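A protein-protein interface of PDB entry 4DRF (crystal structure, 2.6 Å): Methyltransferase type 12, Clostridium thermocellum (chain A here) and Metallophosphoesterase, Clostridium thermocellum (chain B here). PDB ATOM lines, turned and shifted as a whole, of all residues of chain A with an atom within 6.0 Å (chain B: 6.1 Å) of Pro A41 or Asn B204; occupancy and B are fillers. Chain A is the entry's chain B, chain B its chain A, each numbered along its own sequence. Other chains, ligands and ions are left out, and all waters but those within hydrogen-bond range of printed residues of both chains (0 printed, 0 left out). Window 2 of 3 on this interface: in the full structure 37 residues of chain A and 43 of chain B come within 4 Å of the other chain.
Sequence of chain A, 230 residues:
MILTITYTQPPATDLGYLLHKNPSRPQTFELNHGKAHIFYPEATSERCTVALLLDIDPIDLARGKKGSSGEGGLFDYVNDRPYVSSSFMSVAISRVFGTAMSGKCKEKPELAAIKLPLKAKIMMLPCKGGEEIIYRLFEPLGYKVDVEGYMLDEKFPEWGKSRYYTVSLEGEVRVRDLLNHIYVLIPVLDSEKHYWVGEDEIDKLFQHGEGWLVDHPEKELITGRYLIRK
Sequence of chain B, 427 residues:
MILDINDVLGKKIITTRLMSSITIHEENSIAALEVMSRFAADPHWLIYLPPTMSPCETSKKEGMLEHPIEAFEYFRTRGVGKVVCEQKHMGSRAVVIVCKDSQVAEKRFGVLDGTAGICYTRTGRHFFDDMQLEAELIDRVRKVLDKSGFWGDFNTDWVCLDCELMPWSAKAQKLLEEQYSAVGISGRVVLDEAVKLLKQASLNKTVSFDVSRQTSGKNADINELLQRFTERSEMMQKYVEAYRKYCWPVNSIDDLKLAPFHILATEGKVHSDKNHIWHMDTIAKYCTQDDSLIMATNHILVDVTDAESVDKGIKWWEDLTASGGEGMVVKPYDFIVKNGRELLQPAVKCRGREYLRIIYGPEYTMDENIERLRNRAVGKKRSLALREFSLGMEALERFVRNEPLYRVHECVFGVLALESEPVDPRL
ND2 of Asn B204 sits at hydrogen-bond distance from O of Pro A41 (3.1 Å).
Of chain B, only Leu B197, Gln B200, Ala B201 and Asn B204 come within 4 Å of Pro A41. Asn B204 touches just one residue of chain A: Pro A41 (3.1 Å). Of the printed residues of chain B, Tyr A40 touches Ala B201. Of the printed residues of chain A, Gln B200 touches Pro A41 and Glu A42. Of the printed residues of chain A, Ala B201 touches Phe A39 (3.7 Å), Tyr A40 (3.8 Å) and Pro A41 (3.6 Å). Ser B202 touches none of the printed residues of chain A. The nearest printed residue of chain A that does not touch Leu B198 is Pro A41 (5.7 Å).
Of the 9 printed residues of chain B, 5 touch a printed residue of chain A. Printed residues of chain B that touch a printed residue of chain A: Leu B197, Leu B198, Gln B200, Ala B201 and Asn B204. Hydrophobic or aromatic side chains of chain B that line the printed part of chain A: Leu B197, Leu B198 and Ala B201. Among the printed residues, no Asp or Glu carboxylate lies within 4 Å of a Lys or Arg side-chain nitrogen of the other chain.
The backbone carbonyl oxygen (O) of Phe A39 is in hydrogen-bond range of the backbone NH (N) of Ala A51, at 2.8 Å. The backbone carbonyl oxygen of Glu A42 is in hydrogen-bond range of the backbone NH of Thr A49 (2.8 Å). ND2 of Asn B204 is in hydrogen-bond range of O of Gln B200 (3.3 Å).
Among the printed residues, pairs that only touch across the chains: Thr A4 with Leu B197 (3.9 Å), Phe A39 with Leu B197 (3.7 Å), Phe A39 with Leu B198 (3.7 Å), Phe A39 with Ala B201 (3.7 Å), Tyr A40 with Ala B201 (3.8 Å), Pro A41 with Leu B197 (3.7 Å), Pro A41 with Gln B200 (3.6 Å), Pro A41 with Ala B201 (3.6 Å) and Glu A42 with Gln B200 (3.9 Å).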
ATOM      1  N   THR A   4      -3.141 -23.517  18.122  1.00  0.00           N
ATOM      2  CA  THR A   4      -4.086 -23.024  17.143  1.00  0.00           C
ATOM      3  C   THR A   4      -4.234 -24.031  16.015  1.00  0.00           C
ATOM      4  O   THR A   4      -3.281 -24.711  15.657  1.00  0.00           O
ATOM      5  CB  THR A   4      -3.711 -21.638  16.564  1.00  0.00           C
ATOM      6  OG1 THR A   4      -2.432 -21.690  15.933  1.00  0.00           O
ATOM      7  CG2 THR A   4      -3.699 -20.599  17.648  1.00  0.00           C
ATOM      8  N   PHE A  39     -11.704 -20.586  21.920  1.00  0.00           N
ATOM      9  CA  PHE A  39     -12.384 -19.492  21.234  1.00  0.00           C
ATOM     10  C   PHE A  39     -11.843 -19.424  19.807  1.00  0.00           C
ATOM     11  O   PHE A  39     -10.816 -20.022  19.504  1.00  0.00           O
ATOM     12  CB  PHE A  39     -12.166 -18.172  21.977  1.00  0.00           C
ATOM     13  CG  PHE A  39     -10.725 -17.750  22.048  1.00  0.00           C
ATOM     14  CD1 PHE A  39      -9.875 -18.290  22.999  1.00  0.00           C
ATOM     15  CD2 PHE A  39     -10.222 -16.821  21.159  1.00  0.00           C
ATOM     16  CE1 PHE A  39      -8.559 -17.913  23.053  1.00  0.00           C
ATOM     17  CE2 PHE A  39      -8.904 -16.441  21.216  1.00  0.00           C
ATOM     18  CZ  PHE A  39      -8.070 -16.983  22.166  1.00  0.00           C
ATOM     19  N   TYR A  40     -12.545 -18.717  18.931  1.00  0.00           N
ATOM     20  CA  TYR A  40     -12.162 -18.666  17.526  1.00  0.00           C
ATOM     21  C   TYR A  40     -11.736 -17.251  17.160  1.00  0.00           C
ATOM     22  O   TYR A  40     -12.575 -16.381  16.942  1.00  0.00           O
ATOM     23  CB  TYR A  40     -13.328 -19.121  16.623  1.00  0.00           C
ATOM     24  CG  TYR A  40     -13.614 -20.621  16.606  1.00  0.00           C
ATOM     25  CD1 TYR A  40     -13.281 -21.397  15.486  1.00  0.00           C
ATOM     26  CD2 TYR A  40     -14.226 -21.255  17.691  1.00  0.00           C
ATOM     27  CE1 TYR A  40     -13.542 -22.755  15.445  1.00  0.00           C
ATOM     28  CE2 TYR A  40     -14.501 -22.608  17.663  1.00  0.00           C
ATOM     29  CZ  TYR A  40     -14.149 -23.361  16.540  1.00  0.00           C
ATOM     30  OH  TYR A  40     -14.395 -24.723  16.501  1.00  0.00           O
ATOM     31  N   PRO A  41     -10.425 -17.008  17.109  1.00  0.00           N
ATOM     32  CA  PRO A  41      -9.947 -15.671  16.752  1.00  0.00           C
ATOM     33  C   PRO A  41     -10.489 -15.220  15.399  1.00  0.00           C
ATOM     34  O   PRO A  41     -10.713 -14.021  15.189  1.00  0.00           O
ATOM     35  CB  PRO A  41      -8.415 -15.834  16.722  1.00  0.00           C
ATOM     36  CG  PRO A  41      -8.160 -17.321  16.784  1.00  0.00           C
ATOM     37  CD  PRO A  41      -9.326 -17.911  17.484  1.00  0.00           C
ATOM     38  N   GLU A  42     -10.712 -16.180  14.501  1.00  0.00           N
ATOM     39  CA  GLU A  42     -11.258 -15.896  13.172  1.00  0.00           C
ATOM     40  C   GLU A  42     -12.192 -17.000  12.695  1.00  0.00           C
ATOM     41  O   GLU A  42     -11.837 -18.180  12.688  1.00  0.00           O
ATOM     42  CB  GLU A  42     -10.125 -15.696  12.165  1.00  0.00           C
ATOM     43  CG  GLU A  42     -10.574 -15.312  10.767  1.00  0.00           C
ATOM     44  CD  GLU A  42      -9.406 -14.862   9.898  1.00  0.00           C
ATOM     45  OE1 GLU A  42      -8.251 -15.295  10.151  1.00  0.00           O
ATOM     46  OE2 GLU A  42      -9.641 -14.058   8.971  1.00  0.00           O
ATOM     47  N   ALA A  43     -13.397 -16.617  12.296  1.00  0.00           N
ATOM     48  CA  ALA A  43     -14.294 -17.551  11.623  1.00  0.00           C
ATOM     49  C   ALA A  43     -15.037 -16.888  10.470  1.00  0.00           C
ATOM     50  O   ALA A  43     -16.112 -16.321  10.657  1.00  0.00           O
ATOM     51  CB  ALA A  43     -15.265 -18.170  12.593  1.00  0.00           C
ATOM     52  N   THR A  49     -10.005 -20.209  12.368  1.00  0.00           N
ATOM     53  CA  THR A  49      -8.945 -20.624  13.292  1.00  0.00           C
ATOM     54  C   THR A  49      -9.446 -20.851  14.706  1.00  0.00           C
ATOM     55  O   THR A  49     -10.075 -19.995  15.305  1.00  0.00           O
ATOM     56  CB  THR A  49      -7.777 -19.616  13.304  1.00  0.00           C
ATOM     57  OG1 THR A  49      -7.115 -19.618  12.033  1.00  0.00           O
ATOM     58  CG2 THR A  49      -6.762 -19.992  14.352  1.00  0.00           C
ATOM     59  N   VAL A  50      -9.154 -22.016  15.264  1.00  0.00           N
ATOM     60  CA  VAL A  50      -9.527 -22.253  16.652  1.00  0.00           C
ATOM     61  C   VAL A  50      -8.312 -21.985  17.552  1.00  0.00           C
ATOM     62  O   VAL A  50      -7.165 -22.159  17.125  1.00  0.00           O
ATOM     63  CB  VAL A  50     -10.062 -23.677  16.830  1.00  0.00           C
ATOM     64  CG1 VAL A  50      -8.981 -24.680  16.552  1.00  0.00           C
ATOM     65  CG2 VAL A  50     -10.676 -23.880  18.201  1.00  0.00           C
ATOM     66  N   ALA A  51      -8.568 -21.543  18.782  1.00  0.00           N
ATOM     67  CA  ALA A  51      -7.502 -21.269  19.752  1.00  0.00           C
ATOM     68  C   ALA A  51      -7.769 -21.929  21.091  1.00  0.00           C
ATOM     69  O   ALA A  51      -8.829 -21.758  21.697  1.00  0.00           O
ATOM     70  CB  ALA A  51      -7.317 -19.802  19.934  1.00  0.00           C
ATOM     71  N   LEU B 197      -4.335 -12.816  20.002  1.00  0.00           N
ATOM     72  CA  LEU B 197      -5.400 -13.722  19.603  1.00  0.00           C
ATOM     73  C   LEU B 197      -6.777 -13.337  20.146  1.00  0.00           C
ATOM     74  O   LEU B 197      -7.772 -13.363  19.412  1.00  0.00           O
ATOM     75  CB  LEU B 197      -5.047 -15.153  20.015  1.00  0.00           C
ATOM     76  CG  LEU B 197      -3.944 -15.826  19.203  1.00  0.00           C
ATOM     77  CD1 LEU B 197      -3.682 -17.246  19.702  1.00  0.00           C
ATOM     78  CD2 LEU B 197      -4.314 -15.820  17.721  1.00  0.00           C
ATOM     79  N   LEU B 198      -6.832 -13.021  21.434  1.00  0.00           N
ATOM     80  CA  LEU B 198      -8.070 -12.619  22.084  1.00  0.00           C
ATOM     81  C   LEU B 198      -8.592 -11.339  21.451  1.00  0.00           C
ATOM     82  O   LEU B 198      -9.777 -11.216  21.159  1.00  0.00           O
ATOM     83  CB  LEU B 198      -7.824 -12.434  23.586  1.00  0.00           C
ATOM     84  CG  LEU B 198      -7.743 -13.749  24.359  1.00  0.00           C
ATOM     85  CD1 LEU B 198      -7.061 -13.530  25.699  1.00  0.00           C
ATOM     86  CD2 LEU B 198      -9.137 -14.325  24.541  1.00  0.00           C
ATOM     87  N   LYS B 199      -7.684 -10.388  21.263  1.00  0.00           N
ATOM     88  CA  LYS B 199      -7.966  -9.122  20.588  1.00  0.00           C
ATOM     89  C   LYS B 199      -8.611  -9.319  19.216  1.00  0.00           C
ATOM     90  O   LYS B 199      -9.620  -8.702  18.905  1.00  0.00           O
ATOM     91  CB  LYS B 199      -6.671  -8.326  20.430  1.00  0.00           C
ATOM     92  CG  LYS B 199      -6.724  -6.914  20.933  1.00  0.00           C
ATOM     93  CD  LYS B 199      -5.402  -6.174  20.602  1.00  0.00           C
ATOM     94  CE  LYS B 199      -4.511  -5.993  21.832  1.00  0.00           C
ATOM     95  NZ  LYS B 199      -5.321  -5.625  23.054  1.00  0.00           N
ATOM     96  N   GLN B 200      -8.007 -10.171  18.401  1.00  0.00           N
ATOM     97  CA  GLN B 200      -8.557 -10.505  17.088  1.00  0.00           C
ATOM     98  C   GLN B 200      -9.989 -11.026  17.225  1.00  0.00           C
ATOM     99  O   GLN B 200     -10.904 -10.547  16.551  1.00  0.00           O
ATOM    100  CB  GLN B 200      -7.680 -11.549  16.376  1.00  0.00           C
ATOM    101  CG  GLN B 200      -7.974 -11.731  14.917  1.00  0.00           C
ATOM    102  CD  GLN B 200      -7.076 -12.771  14.265  1.00  0.00           C
ATOM    103  OE1 GLN B 200      -6.354 -13.487  14.943  1.00  0.00           O
ATOM    104  NE2 GLN B 200      -7.125 -12.861  12.941  1.00  0.00           N
ATOM    105  N   ALA B 201     -10.170 -11.978  18.140  1.00  0.00           N
ATOM    106  CA  ALA B 201     -11.482 -12.566  18.429  1.00  0.00           C
ATOM    107  C   ALA B 201     -12.452 -11.535  18.987  1.00  0.00           C
ATOM    108  O   ALA B 201     -13.650 -11.604  18.732  1.00  0.00           O
ATOM    109  CB  ALA B 201     -11.334 -13.733  19.397  1.00  0.00           C
ATOM    110  N   SER B 202     -11.922 -10.591  19.762  1.00  0.00           N
ATOM    111  CA  SER B 202     -12.702  -9.483  20.289  1.00  0.00           C
ATOM    112  C   SER B 202     -13.311  -8.689  19.128  1.00  0.00           C
ATOM    113  O   SER B 202     -14.479  -8.313  19.173  1.00  0.00           O
ATOM    114  CB  SER B 202     -11.819  -8.578  21.148  1.00  0.00           C
ATOM    115  OG  SER B 202     -12.513  -7.440  21.632  1.00  0.00           O
ATOM    116  N   LEU B 203     -12.522  -8.455  18.085  1.00  0.00           N
ATOM    117  CA  LEU B 203     -12.968  -7.652  16.957  1.00  0.00           C
ATOM    118  C   LEU B 203     -13.798  -8.462  15.954  1.00  0.00           C
ATOM    119  O   LEU B 203     -14.595  -7.898  15.203  1.00  0.00           O
ATOM    120  CB  LEU B 203     -11.781  -6.958  16.269  1.00  0.00           C
ATOM    121  CG  LEU B 203     -10.923  -6.040  17.166  1.00  0.00           C
ATOM    122  CD1 LEU B 203      -9.869  -5.259  16.356  1.00  0.00           C
ATOM    123  CD2 LEU B 203     -11.775  -5.091  18.023  1.00  0.00           C
ATOM    124  N   ASN B 204     -13.630  -9.782  15.955  1.00  0.00           N
ATOM    125  CA  ASN B 204     -14.339 -10.644  15.000  1.00  0.00           C
ATOM    126  C   ASN B 204     -15.483 -11.431  15.636  1.00  0.00           C
ATOM    127  O   ASN B 204     -15.719 -12.585  15.291  1.00  0.00           O
ATOM    128  CB  ASN B 204     -13.378 -11.639  14.329  1.00  0.00           C
ATOM    129  CG  ASN B 204     -12.329 -10.964  13.455  1.00  0.00           C
ATOM    130  OD1 ASN B 204     -12.585  -9.941  12.824  1.00  0.00           O
ATOM    131  ND2 ASN B 204     -11.136 -11.545  13.417  1.00  0.00           N
ATOM    132  N   LYS B 205     -16.196 -10.798  16.555  1.00  0.00           N
ATOM    133  CA  LYS B 205     -17.169 -11.489  17.374  1.00  0.00           C
ATOM    134  C   LYS B 205     -18.594 -11.100  17.014  1.00  0.00           C
ATOM    135  O   LYS B 205     -18.822 -10.212  16.206  1.00  0.00           O
ATOM    136  CB  LYS B 205     -16.869 -11.219  18.849  1.00  0.00           C
ATOM    137  CG  LYS B 205     -18.087 -10.932  19.715  1.00  0.00           C
ATOM    138  CD  LYS B 205     -17.681 -10.773  21.178  1.00  0.00           C
ATOM    139  CE  LYS B 205     -18.817 -11.166  22.099  1.00  0.00           C
ATOM    140  NZ  LYS B 205     -19.370  -9.997  22.821  1.00  0.00           N
